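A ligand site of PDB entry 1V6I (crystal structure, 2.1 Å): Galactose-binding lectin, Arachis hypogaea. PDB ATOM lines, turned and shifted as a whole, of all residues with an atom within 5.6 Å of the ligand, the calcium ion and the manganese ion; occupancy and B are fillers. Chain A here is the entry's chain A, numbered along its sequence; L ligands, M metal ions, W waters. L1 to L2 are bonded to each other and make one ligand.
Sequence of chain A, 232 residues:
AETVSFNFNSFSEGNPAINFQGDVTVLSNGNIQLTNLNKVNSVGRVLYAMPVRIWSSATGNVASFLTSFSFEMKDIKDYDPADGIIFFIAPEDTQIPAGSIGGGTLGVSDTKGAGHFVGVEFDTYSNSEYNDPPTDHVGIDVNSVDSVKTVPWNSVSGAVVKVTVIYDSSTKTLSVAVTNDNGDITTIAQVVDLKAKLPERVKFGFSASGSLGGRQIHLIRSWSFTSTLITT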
ATOM      1  N   ASP A  80      20.736  33.343  28.968  1.00  0.00           N
ATOM      2  CA  ASP A  80      20.172  33.514  27.637  1.00  0.00           C
ATOM      3  C   ASP A  80      18.661  33.414  27.805  1.00  0.00           C
ATOM      4  O   ASP A  80      18.174  32.633  28.617  1.00  0.00           O
ATOM      5  CB  ASP A  80      20.606  32.373  26.729  1.00  0.00           C
ATOM      6  CG  ASP A  80      21.716  32.770  25.792  1.00  0.00           C
ATOM      7  OD1 ASP A  80      22.773  33.231  26.276  1.00  0.00           O
ATOM      8  OD2 ASP A  80      21.520  32.607  24.573  1.00  0.00           O
ATOM      9  N   ALA A  82      15.204  32.577  25.661  1.00  0.00           N
ATOM     10  CA  ALA A  82      15.227  31.308  26.404  1.00  0.00           C
ATOM     11  C   ALA A  82      14.203  31.048  27.515  1.00  0.00           C
ATOM     12  O   ALA A  82      14.401  31.477  28.653  1.00  0.00           O
ATOM     13  CB  ALA A  82      16.617  31.042  26.913  1.00  0.00           C
ATOM     14  N   ASP A  83      13.132  30.309  27.208  1.00  0.00           N
ATOM     15  CA  ASP A  83      12.879  29.722  25.883  1.00  0.00           C
ATOM     16  C   ASP A  83      11.587  30.231  25.253  1.00  0.00           C
ATOM     17  O   ASP A  83      11.431  30.212  24.028  1.00  0.00           O
ATOM     18  CB  ASP A  83      12.818  28.202  25.979  1.00  0.00           C
ATOM     19  CG  ASP A  83      14.166  27.542  25.751  1.00  0.00           C
ATOM     20  OD1 ASP A  83      14.571  27.409  24.587  1.00  0.00           O
ATOM     21  OD2 ASP A  83      14.816  27.159  26.747  1.00  0.00           O
ATOM     22  N   GLY A 103      13.754  23.565  27.961  1.00  0.00           N
ATOM     23  CA  GLY A 103      14.332  24.198  26.798  1.00  0.00           C
ATOM     24  C   GLY A 103      13.384  24.417  25.631  1.00  0.00           C
ATOM     25  O   GLY A 103      12.258  24.893  25.815  1.00  0.00           O
ATOM     26  N   GLY A 104      13.836  24.045  24.435  1.00  0.00           N
ATOM     27  CA  GLY A 104      13.039  24.206  23.237  1.00  0.00           C
ATOM     28  C   GLY A 104      11.767  23.379  23.120  1.00  0.00           C
ATOM     29  O   GLY A 104      10.976  23.601  22.205  1.00  0.00           O
ATOM     30  N   LEU A 106       9.471  23.529  25.133  1.00  0.00           N
ATOM     31  CA  LEU A 106       8.478  24.411  25.713  1.00  0.00           C
ATOM     32  C   LEU A 106       7.567  23.757  26.749  1.00  0.00           C
ATOM     33  O   LEU A 106       6.474  24.258  27.046  1.00  0.00           O
ATOM     34  CB  LEU A 106       7.639  25.060  24.584  1.00  0.00           C
ATOM     35  CG  LEU A 106       8.479  25.942  23.641  1.00  0.00           C
ATOM     36  CD1 LEU A 106       7.616  26.527  22.541  1.00  0.00           C
ATOM     37  CD2 LEU A 106       9.128  27.058  24.432  1.00  0.00           C
ATOM     38  N   GLU A 121       2.792  29.303  19.882  1.00  0.00           N
ATOM     39  CA  GLU A 121       4.017  29.581  20.621  1.00  0.00           C
ATOM     40  C   GLU A 121       4.608  30.964  20.386  1.00  0.00           C
ATOM     41  O   GLU A 121       4.480  31.555  19.300  1.00  0.00           O
ATOM     42  CB  GLU A 121       5.075  28.517  20.301  1.00  0.00           C
ATOM     43  CG  GLU A 121       5.449  28.437  18.839  1.00  0.00           C
ATOM     44  CD  GLU A 121       6.712  27.635  18.599  1.00  0.00           C
ATOM     45  OE1 GLU A 121       6.753  26.448  18.957  1.00  0.00           O
ATOM     46  OE2 GLU A 121       7.668  28.212  18.050  1.00  0.00           O
ATOM     47  N   ASP A 123       8.037  31.971  20.762  1.00  0.00           N
ATOM     48  CA  ASP A 123       9.371  31.420  20.850  1.00  0.00           C
ATOM     49  C   ASP A 123      10.526  32.425  20.822  1.00  0.00           C
ATOM     50  O   ASP A 123      10.703  33.128  19.829  1.00  0.00           O
ATOM     51  CB  ASP A 123       9.522  30.437  19.694  1.00  0.00           C
ATOM     52  CG  ASP A 123      10.521  29.389  19.986  1.00  0.00           C
ATOM     53  OD1 ASP A 123      11.466  29.675  20.747  1.00  0.00           O
ATOM     54  OD2 ASP A 123      10.361  28.273  19.446  1.00  0.00           O
ATOM     55  N   THR A 124      11.330  32.442  21.882  1.00  0.00           N
ATOM     56  CA  THR A 124      12.440  33.395  21.964  1.00  0.00           C
ATOM     57  C   THR A 124      13.848  32.848  21.728  1.00  0.00           C
ATOM     58  O   THR A 124      14.819  33.564  21.903  1.00  0.00           O
ATOM     59  CB  THR A 124      12.444  34.107  23.332  1.00  0.00           C
ATOM     60  OG1 THR A 124      12.807  33.167  24.347  1.00  0.00           O
ATOM     61  CG2 THR A 124      11.062  34.678  23.639  1.00  0.00           C
ATOM     62  N   TYR A 125      13.965  31.587  21.354  1.00  0.00           N
ATOM     63  CA  TYR A 125      15.298  31.021  21.087  1.00  0.00           C
ATOM     64  C   TYR A 125      15.230  30.109  19.875  1.00  0.00           C
ATOM     65  O   TYR A 125      14.285  29.348  19.732  1.00  0.00           O
ATOM     66  CB  TYR A 125      15.824  30.245  22.296  1.00  0.00           C
ATOM     67  CG  TYR A 125      17.160  29.602  22.018  1.00  0.00           C
ATOM     68  CD1 TYR A 125      17.236  28.355  21.389  1.00  0.00           C
ATOM     69  CD2 TYR A 125      18.356  30.264  22.320  1.00  0.00           C
ATOM     70  CE1 TYR A 125      18.459  27.788  21.062  1.00  0.00           C
ATOM     71  CE2 TYR A 125      19.587  29.703  21.997  1.00  0.00           C
ATOM     72  CZ  TYR A 125      19.631  28.468  21.368  1.00  0.00           C
ATOM     73  OH  TYR A 125      20.838  27.907  21.041  1.00  0.00           O
ATOM     74  N   SER A 126      16.228  30.159  19.009  1.00  0.00           N
ATOM     75  CA  SER A 126      16.187  29.336  17.812  1.00  0.00           C
ATOM     76  C   SER A 126      16.812  27.954  17.935  1.00  0.00           C
ATOM     77  O   SER A 126      18.027  27.807  17.857  1.00  0.00           O
ATOM     78  CB  SER A 126      16.845  30.099  16.661  1.00  0.00           C
ATOM     79  OG  SER A 126      16.845  29.321  15.477  1.00  0.00           O
ATOM     80  N   ASN A 127      15.964  26.937  18.134  1.00  0.00           N
ATOM     81  CA  ASN A 127      16.447  25.555  18.238  1.00  0.00           C
ATOM     82  C   ASN A 127      16.458  24.964  16.842  1.00  0.00           C
ATOM     83  O   ASN A 127      15.406  24.662  16.275  1.00  0.00           O
ATOM     84  CB  ASN A 127      15.528  24.690  19.111  1.00  0.00           C
ATOM     85  CG  ASN A 127      15.482  25.138  20.553  1.00  0.00           C
ATOM     86  OD1 ASN A 127      14.789  26.089  20.889  1.00  0.00           O
ATOM     87  ND2 ASN A 127      16.236  24.466  21.410  1.00  0.00           N
ATOM     88  N   GLU A 129      17.316  22.085  16.036  1.00  0.00           N
ATOM     89  CA  GLU A 129      16.874  20.695  16.074  1.00  0.00           C
ATOM     90  C   GLU A 129      15.354  20.588  15.842  1.00  0.00           C
ATOM     91  O   GLU A 129      14.848  19.497  15.572  1.00  0.00           O
ATOM     92  CB  GLU A 129      17.245  20.020  17.396  1.00  0.00           C
ATOM     93  CG  GLU A 129      16.582  20.624  18.628  1.00  0.00           C
ATOM     94  CD  GLU A 129      17.423  21.721  19.280  1.00  0.00           C
ATOM     95  OE1 GLU A 129      18.134  22.445  18.548  1.00  0.00           O
ATOM     96  OE2 GLU A 129      17.355  21.869  20.515  1.00  0.00           O
ATOM     97  N   TYR A 130      14.651  21.703  15.960  1.00  0.00           N
ATOM     98  CA  TYR A 130      13.191  21.711  15.746  1.00  0.00           C
ATOM     99  C   TYR A 130      12.855  22.616  14.561  1.00  0.00           C
ATOM    100  O   TYR A 130      11.732  23.086  14.427  1.00  0.00           O
ATOM    101  CB  TYR A 130      12.463  22.205  16.994  1.00  0.00           C
ATOM    102  CG  TYR A 130      12.762  21.401  18.234  1.00  0.00           C
ATOM    103  CD1 TYR A 130      12.661  20.018  18.237  1.00  0.00           C
ATOM    104  CD2 TYR A 130      13.187  22.028  19.412  1.00  0.00           C
ATOM    105  CE1 TYR A 130      12.982  19.267  19.363  1.00  0.00           C
ATOM    106  CE2 TYR A 130      13.496  21.282  20.555  1.00  0.00           C
ATOM    107  CZ  TYR A 130      13.398  19.903  20.520  1.00  0.00           C
ATOM    108  OH  TYR A 130      13.726  19.155  21.626  1.00  0.00           O
ATOM    109  N   ASP A 132      13.569  25.692  13.871  1.00  0.00           N
ATOM    110  CA  ASP A 132      13.108  27.034  14.203  1.00  0.00           C
ATOM    111  C   ASP A 132      13.605  28.087  13.228  1.00  0.00           C
ATOM    112  O   ASP A 132      14.656  27.922  12.612  1.00  0.00           O
ATOM    113  CB  ASP A 132      13.623  27.465  15.576  1.00  0.00           C
ATOM    114  CG  ASP A 132      12.718  27.064  16.699  1.00  0.00           C
ATOM    115  OD1 ASP A 132      11.494  26.977  16.484  1.00  0.00           O
ATOM    116  OD2 ASP A 132      13.230  26.860  17.808  1.00  0.00           O
ATOM    117  N   PRO A 133      12.850  29.183  13.081  1.00  0.00           N
ATOM    118  CA  PRO A 133      13.308  30.232  12.168  1.00  0.00           C
ATOM    119  C   PRO A 133      14.505  30.830  12.900  1.00  0.00           C
ATOM    120  O   PRO A 133      14.723  30.536  14.078  1.00  0.00           O
ATOM    121  CB  PRO A 133      12.120  31.193  12.123  1.00  0.00           C
ATOM    122  CG  PRO A 133      10.950  30.308  12.402  1.00  0.00           C
ATOM    123  CD  PRO A 133      11.461  29.424  13.511  1.00  0.00           C
ATOM    124  N   HIS A 137       9.898  34.303  17.171  1.00  0.00           N
ATOM    125  CA  HIS A 137       8.755  34.091  16.305  1.00  0.00           C
ATOM    126  C   HIS A 137       7.505  33.572  17.000  1.00  0.00           C
ATOM    127  O   HIS A 137       7.535  33.103  18.133  1.00  0.00           O
ATOM    128  CB  HIS A 137       9.129  33.082  15.218  1.00  0.00           C
ATOM    129  CG  HIS A 137       9.690  31.812  15.761  1.00  0.00           C
ATOM    130  ND1 HIS A 137      10.974  31.722  16.268  1.00  0.00           N
ATOM    131  CD2 HIS A 137       9.126  30.597  15.936  1.00  0.00           C
ATOM    132  CE1 HIS A 137      11.164  30.494  16.737  1.00  0.00           C
ATOM    133  NE2 HIS A 137      10.064  29.795  16.546  1.00  0.00           N
ATOM    134  N   VAL A 145       6.776  20.833  18.146  1.00  0.00           N
ATOM    135  CA  VAL A 145       7.299  22.183  18.310  1.00  0.00           C
ATOM    136  C   VAL A 145       7.966  22.601  17.000  1.00  0.00           C
ATOM    137  O   VAL A 145       8.532  23.690  16.877  1.00  0.00           O
ATOM    138  CB  VAL A 145       8.310  22.281  19.470  1.00  0.00           C
ATOM    139  CG1 VAL A 145       7.574  22.178  20.811  1.00  0.00           C
ATOM    140  CG2 VAL A 145       9.359  21.203  19.347  1.00  0.00           C
ATOM    141  N   SER A 147       7.009  23.878  14.235  1.00  0.00           N
ATOM    142  CA  SER A 147       5.822  24.592  13.759  1.00  0.00           C
ATOM    143  C   SER A 147       5.383  24.332  12.322  1.00  0.00           C
ATOM    144  O   SER A 147       6.188  24.224  11.402  1.00  0.00           O
ATOM    145  CB  SER A 147       6.022  26.102  13.944  1.00  0.00           C
ATOM    146  OG  SER A 147       6.252  26.427  15.310  1.00  0.00           O
ATOM    147  N   THR A 150       5.134  29.695  10.917  1.00  0.00           N
ATOM    148  CA  THR A 150       5.677  30.713  11.816  1.00  0.00           C
ATOM    149  C   THR A 150       5.684  32.066  11.142  1.00  0.00           C
ATOM    150  O   THR A 150       5.563  32.155   9.918  1.00  0.00           O
ATOM    151  CB  THR A 150       7.132  30.419  12.253  1.00  0.00           C
ATOM    152  OG1 THR A 150       8.001  30.560  11.113  1.00  0.00           O
ATOM    153  CG2 THR A 150       7.259  29.009  12.823  1.00  0.00           C
ATOM    154  N   GLY A 210      12.851  26.455  30.346  1.00  0.00           N
ATOM    155  CA  GLY A 210      14.182  26.999  30.168  1.00  0.00           C
ATOM    156  C   GLY A 210      15.194  25.877  30.208  1.00  0.00           C
ATOM    157  O   GLY A 210      14.818  24.703  30.359  1.00  0.00           O
ATOM    158  N   SER A 211      16.476  26.207  30.064  1.00  0.00           N
ATOM    159  CA  SER A 211      17.538  25.201  30.088  1.00  0.00           C
ATOM    160  C   SER A 211      18.565  25.603  31.140  1.00  0.00           C
ATOM    161  O   SER A 211      18.290  26.426  32.017  1.00  0.00           O
ATOM    162  CB  SER A 211      18.207  25.107  28.714  1.00  0.00           C
ATOM    163  OG  SER A 211      18.817  26.338  28.341  1.00  0.00           O
ATOM    164  N   LEU A 212      19.767  25.023  31.063  1.00  0.00           N
ATOM    165  CA  LEU A 212      20.800  25.357  32.029  1.00  0.00           C
ATOM    166  C   LEU A 212      21.274  26.789  31.764  1.00  0.00           C
ATOM    167  O   LEU A 212      21.397  27.587  32.688  1.00  0.00           O
ATOM    168  CB  LEU A 212      21.985  24.380  31.916  1.00  0.00           C
ATOM    169  CG  LEU A 212      23.101  24.506  32.951  1.00  0.00           C
ATOM    170  CD1 LEU A 212      23.891  23.218  33.006  1.00  0.00           C
ATOM    171  CD2 LEU A 212      23.999  25.686  32.623  1.00  0.00           C
ATOM    172  N   GLY A 213      21.520  27.101  30.491  1.00  0.00           N
ATOM    173  CA  GLY A 213      21.977  28.436  30.146  1.00  0.00           C
ATOM    174  C   GLY A 213      20.870  29.387  29.725  1.00  0.00           C
ATOM    175  O   GLY A 213      21.060  30.595  29.736  1.00  0.00           O
ATOM    176  N   GLY A 214      19.724  28.837  29.333  1.00  0.00           N
ATOM    177  CA  GLY A 214      18.618  29.674  28.898  1.00  0.00           C
ATOM    178  C   GLY A 214      17.543  29.824  29.961  1.00  0.00           C
ATOM    179  O   GLY A 214      16.874  28.864  30.322  1.00  0.00           O
HETATM  180  C1  LIG L   1      24.618  23.541  26.957  1.00  0.00           C
HETATM  181  C2  LIG L   1      23.921  24.728  27.639  1.00  0.00           C
HETATM  182  C3  LIG L   1      22.403  24.646  27.451  1.00  0.00           C
HETATM  183  C4  LIG L   1      22.067  24.496  25.973  1.00  0.00           C
HETATM  184  C5  LIG L   1      22.804  23.272  25.416  1.00  0.00           C
HETATM  185  C6  LIG L   1      22.541  23.020  23.944  1.00  0.00           C
HETATM  186  O1  LIG L   1      24.257  22.363  27.591  1.00  0.00           O
HETATM  187  O2  LIG L   1      24.226  24.709  29.024  1.00  0.00           O
HETATM  188  O3  LIG L   1      21.793  25.827  27.957  1.00  0.00           O
HETATM  189  O4  LIG L   1      20.648  24.334  25.814  1.00  0.00           O
HETATM  190  O5  LIG L   1      24.223  23.435  25.575  1.00  0.00           O
HETATM  191  O6  LIG L   1      22.765  24.189  23.185  1.00  0.00           O
HETATM  192  C1  LG2 L   2      20.002  25.248  25.003  1.00  0.00           C
HETATM  193  C2  LG2 L   2      18.535  24.841  24.863  1.00  0.00           C
HETATM  194  C3  LG2 L   2      17.734  25.924  24.133  1.00  0.00           C
HETATM  195  C4  LG2 L   2      17.939  27.282  24.826  1.00  0.00           C
HETATM  196  C5  LG2 L   2      19.438  27.573  24.863  1.00  0.00           C
HETATM  197  C6  LG2 L   2      19.768  28.905  25.512  1.00  0.00           C
HETATM  198  O1  LG2 L   2      18.446  23.626  24.139  1.00  0.00           O
HETATM  199  O2  LG2 L   2      16.363  25.580  24.135  1.00  0.00           O
HETATM  200  O3  LG2 L   2      17.431  27.230  26.155  1.00  0.00           O
HETATM  201  O4  LG2 L   2      20.106  26.548  25.611  1.00  0.00           O
HETATM  202  O5  LG2 L   2      21.055  29.353  25.124  1.00  0.00           O
HETATM  203 CA    CA M   1      12.744  27.472  20.208  1.00  0.00          CA
HETATM  204 MN    MN M   2       9.681  27.703  17.424  1.00  0.00          MN
HETATM  205  O   HOH W   1       8.785  27.083  15.361  1.00  0.00           O
HETATM  206  O   HOH W   2      19.325  23.348  21.438  1.00  0.00           O
HETATM  207  O   HOH W   3      22.615  28.252  26.921  1.00  0.00           O
HETATM  208  O   HOH W   4      11.270  25.377  20.239  1.00  0.00           O
HETATM  209  O   HOH W   5      26.465  26.857  29.794  1.00  0.00           O
HETATM  210  O   HOH W   6       9.231  25.670  18.474  1.00  0.00           O
HETATM  211  O   HOH W   7      19.518  21.680  26.915  1.00  0.00           O
HETATM  212  O   HOH W   8      12.757  27.907  22.746  1.00  0.00           O
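The manganese ion is bound by OD1 of Asp 132 (2.2 Å), OE2 of Glu 121 (2.2 Å), OD2 of Asp 123 (2.2 Å), NE2 of His 137 (2.3 Å), water W1 (2.3 Å) and water W6 (2.3 Å).
An oxygen (O2) of LG2 L2 is in hydrogen-bond range of the side-chain carboxylate (OD1) of Asp 83, 2.6 Å away.
The backbone NH (N) of Gly 104 lies within hydrogen-bond range of an oxygen (O2) of LG2 L2, 3.0 Å away.
The backbone NH (N) of Gly 213 is in hydrogen-bond range of an oxygen (O3) of LIG L1, at 2.8 Å.
The side-chain carboxylate (OD2) of Asp 80 sits at hydrogen-bond distance from an oxygen (O5) of LG2 L2 (3.3 Å).
OG of Ser 211 lies within hydrogen-bond range of O3 of LG2 L2 (2.7 Å).
An oxygen (O2) of LG2 L2 is in hydrogen-bond range of the side-chain amide nitrogen (ND2) of Asn 127, at 2.9 Å.
Water W6 lies within hydrogen-bond range of the backbone carbonyl oxygen (O) of Val 145 (2.6 Å) and the side-chain carboxylate (OE1) of Glu 121 (2.6 Å).
Water W2 lies within hydrogen-bond range of the side-chain carboxylate of Glu 129 (2.6 Å), an oxygen (O1) of LG2 L2 (2.9 Å) and the side-chain amide nitrogen of Asn 127 (3.3 Å).
The side-chain hydroxyl (OG) of Ser 211 lies within hydrogen-bond range of the backbone NH (N) of Gly 214, at 2.8 Å.
OE2 of Glu 129 sits at hydrogen-bond distance from ND2 of Asn 127 (3.0 Å).
The side-chain carboxylate of Asp 83 sits at hydrogen-bond distance from the backbone NH of Gly 104 (3.4 Å).
The backbone carbonyl oxygen (O) of Asp 83 is in hydrogen-bond range of the backbone NH (N) of Thr 124, at 3.1 Å.
N of Gly 103 lies within hydrogen-bond range of O of Gly 210 (2.9 Å).
N of Asp 80 sits at hydrogen-bond distance from O of Gly 213 (2.9 Å).
N of Ala 82 lies within hydrogen-bond range of OG1 of Thr 124.
Residues that only touch the ligand: Gly 103 (3.5 Å), Gly 214 (3.7 Å), Leu 212 (3.7 Å) and Ala 82 (3.97 Å).
Hydrophobic or aromatic side chains that line the ligand: Ala 82, Tyr 125 and Leu 212.
The nearest printed residue that does not touch the manganese ion is Val 145 (4.2 Å).
The calcium ion is bound by the backbone carbonyl oxygen (O) of Tyr 125 (2.5 Å), the side-chain carboxylate (OD2) of Asp 132 (2.5 Å), the side-chain amide oxygen (OD1) of Asn 127 (2.6 Å), water W4 (2.6 Å), water W8 (2.6 Å), the side-chain carboxylate (OD1) of Asp 123 (2.6 Å) and the side-chain carboxylate (OD2) of Asp 123 (2.6 Å).
The calcium ion has seven donor atoms within binding distance.
Within 4 Å of the calcium ion: Asp 123, Tyr 125, Asn 127 and Asp 132.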
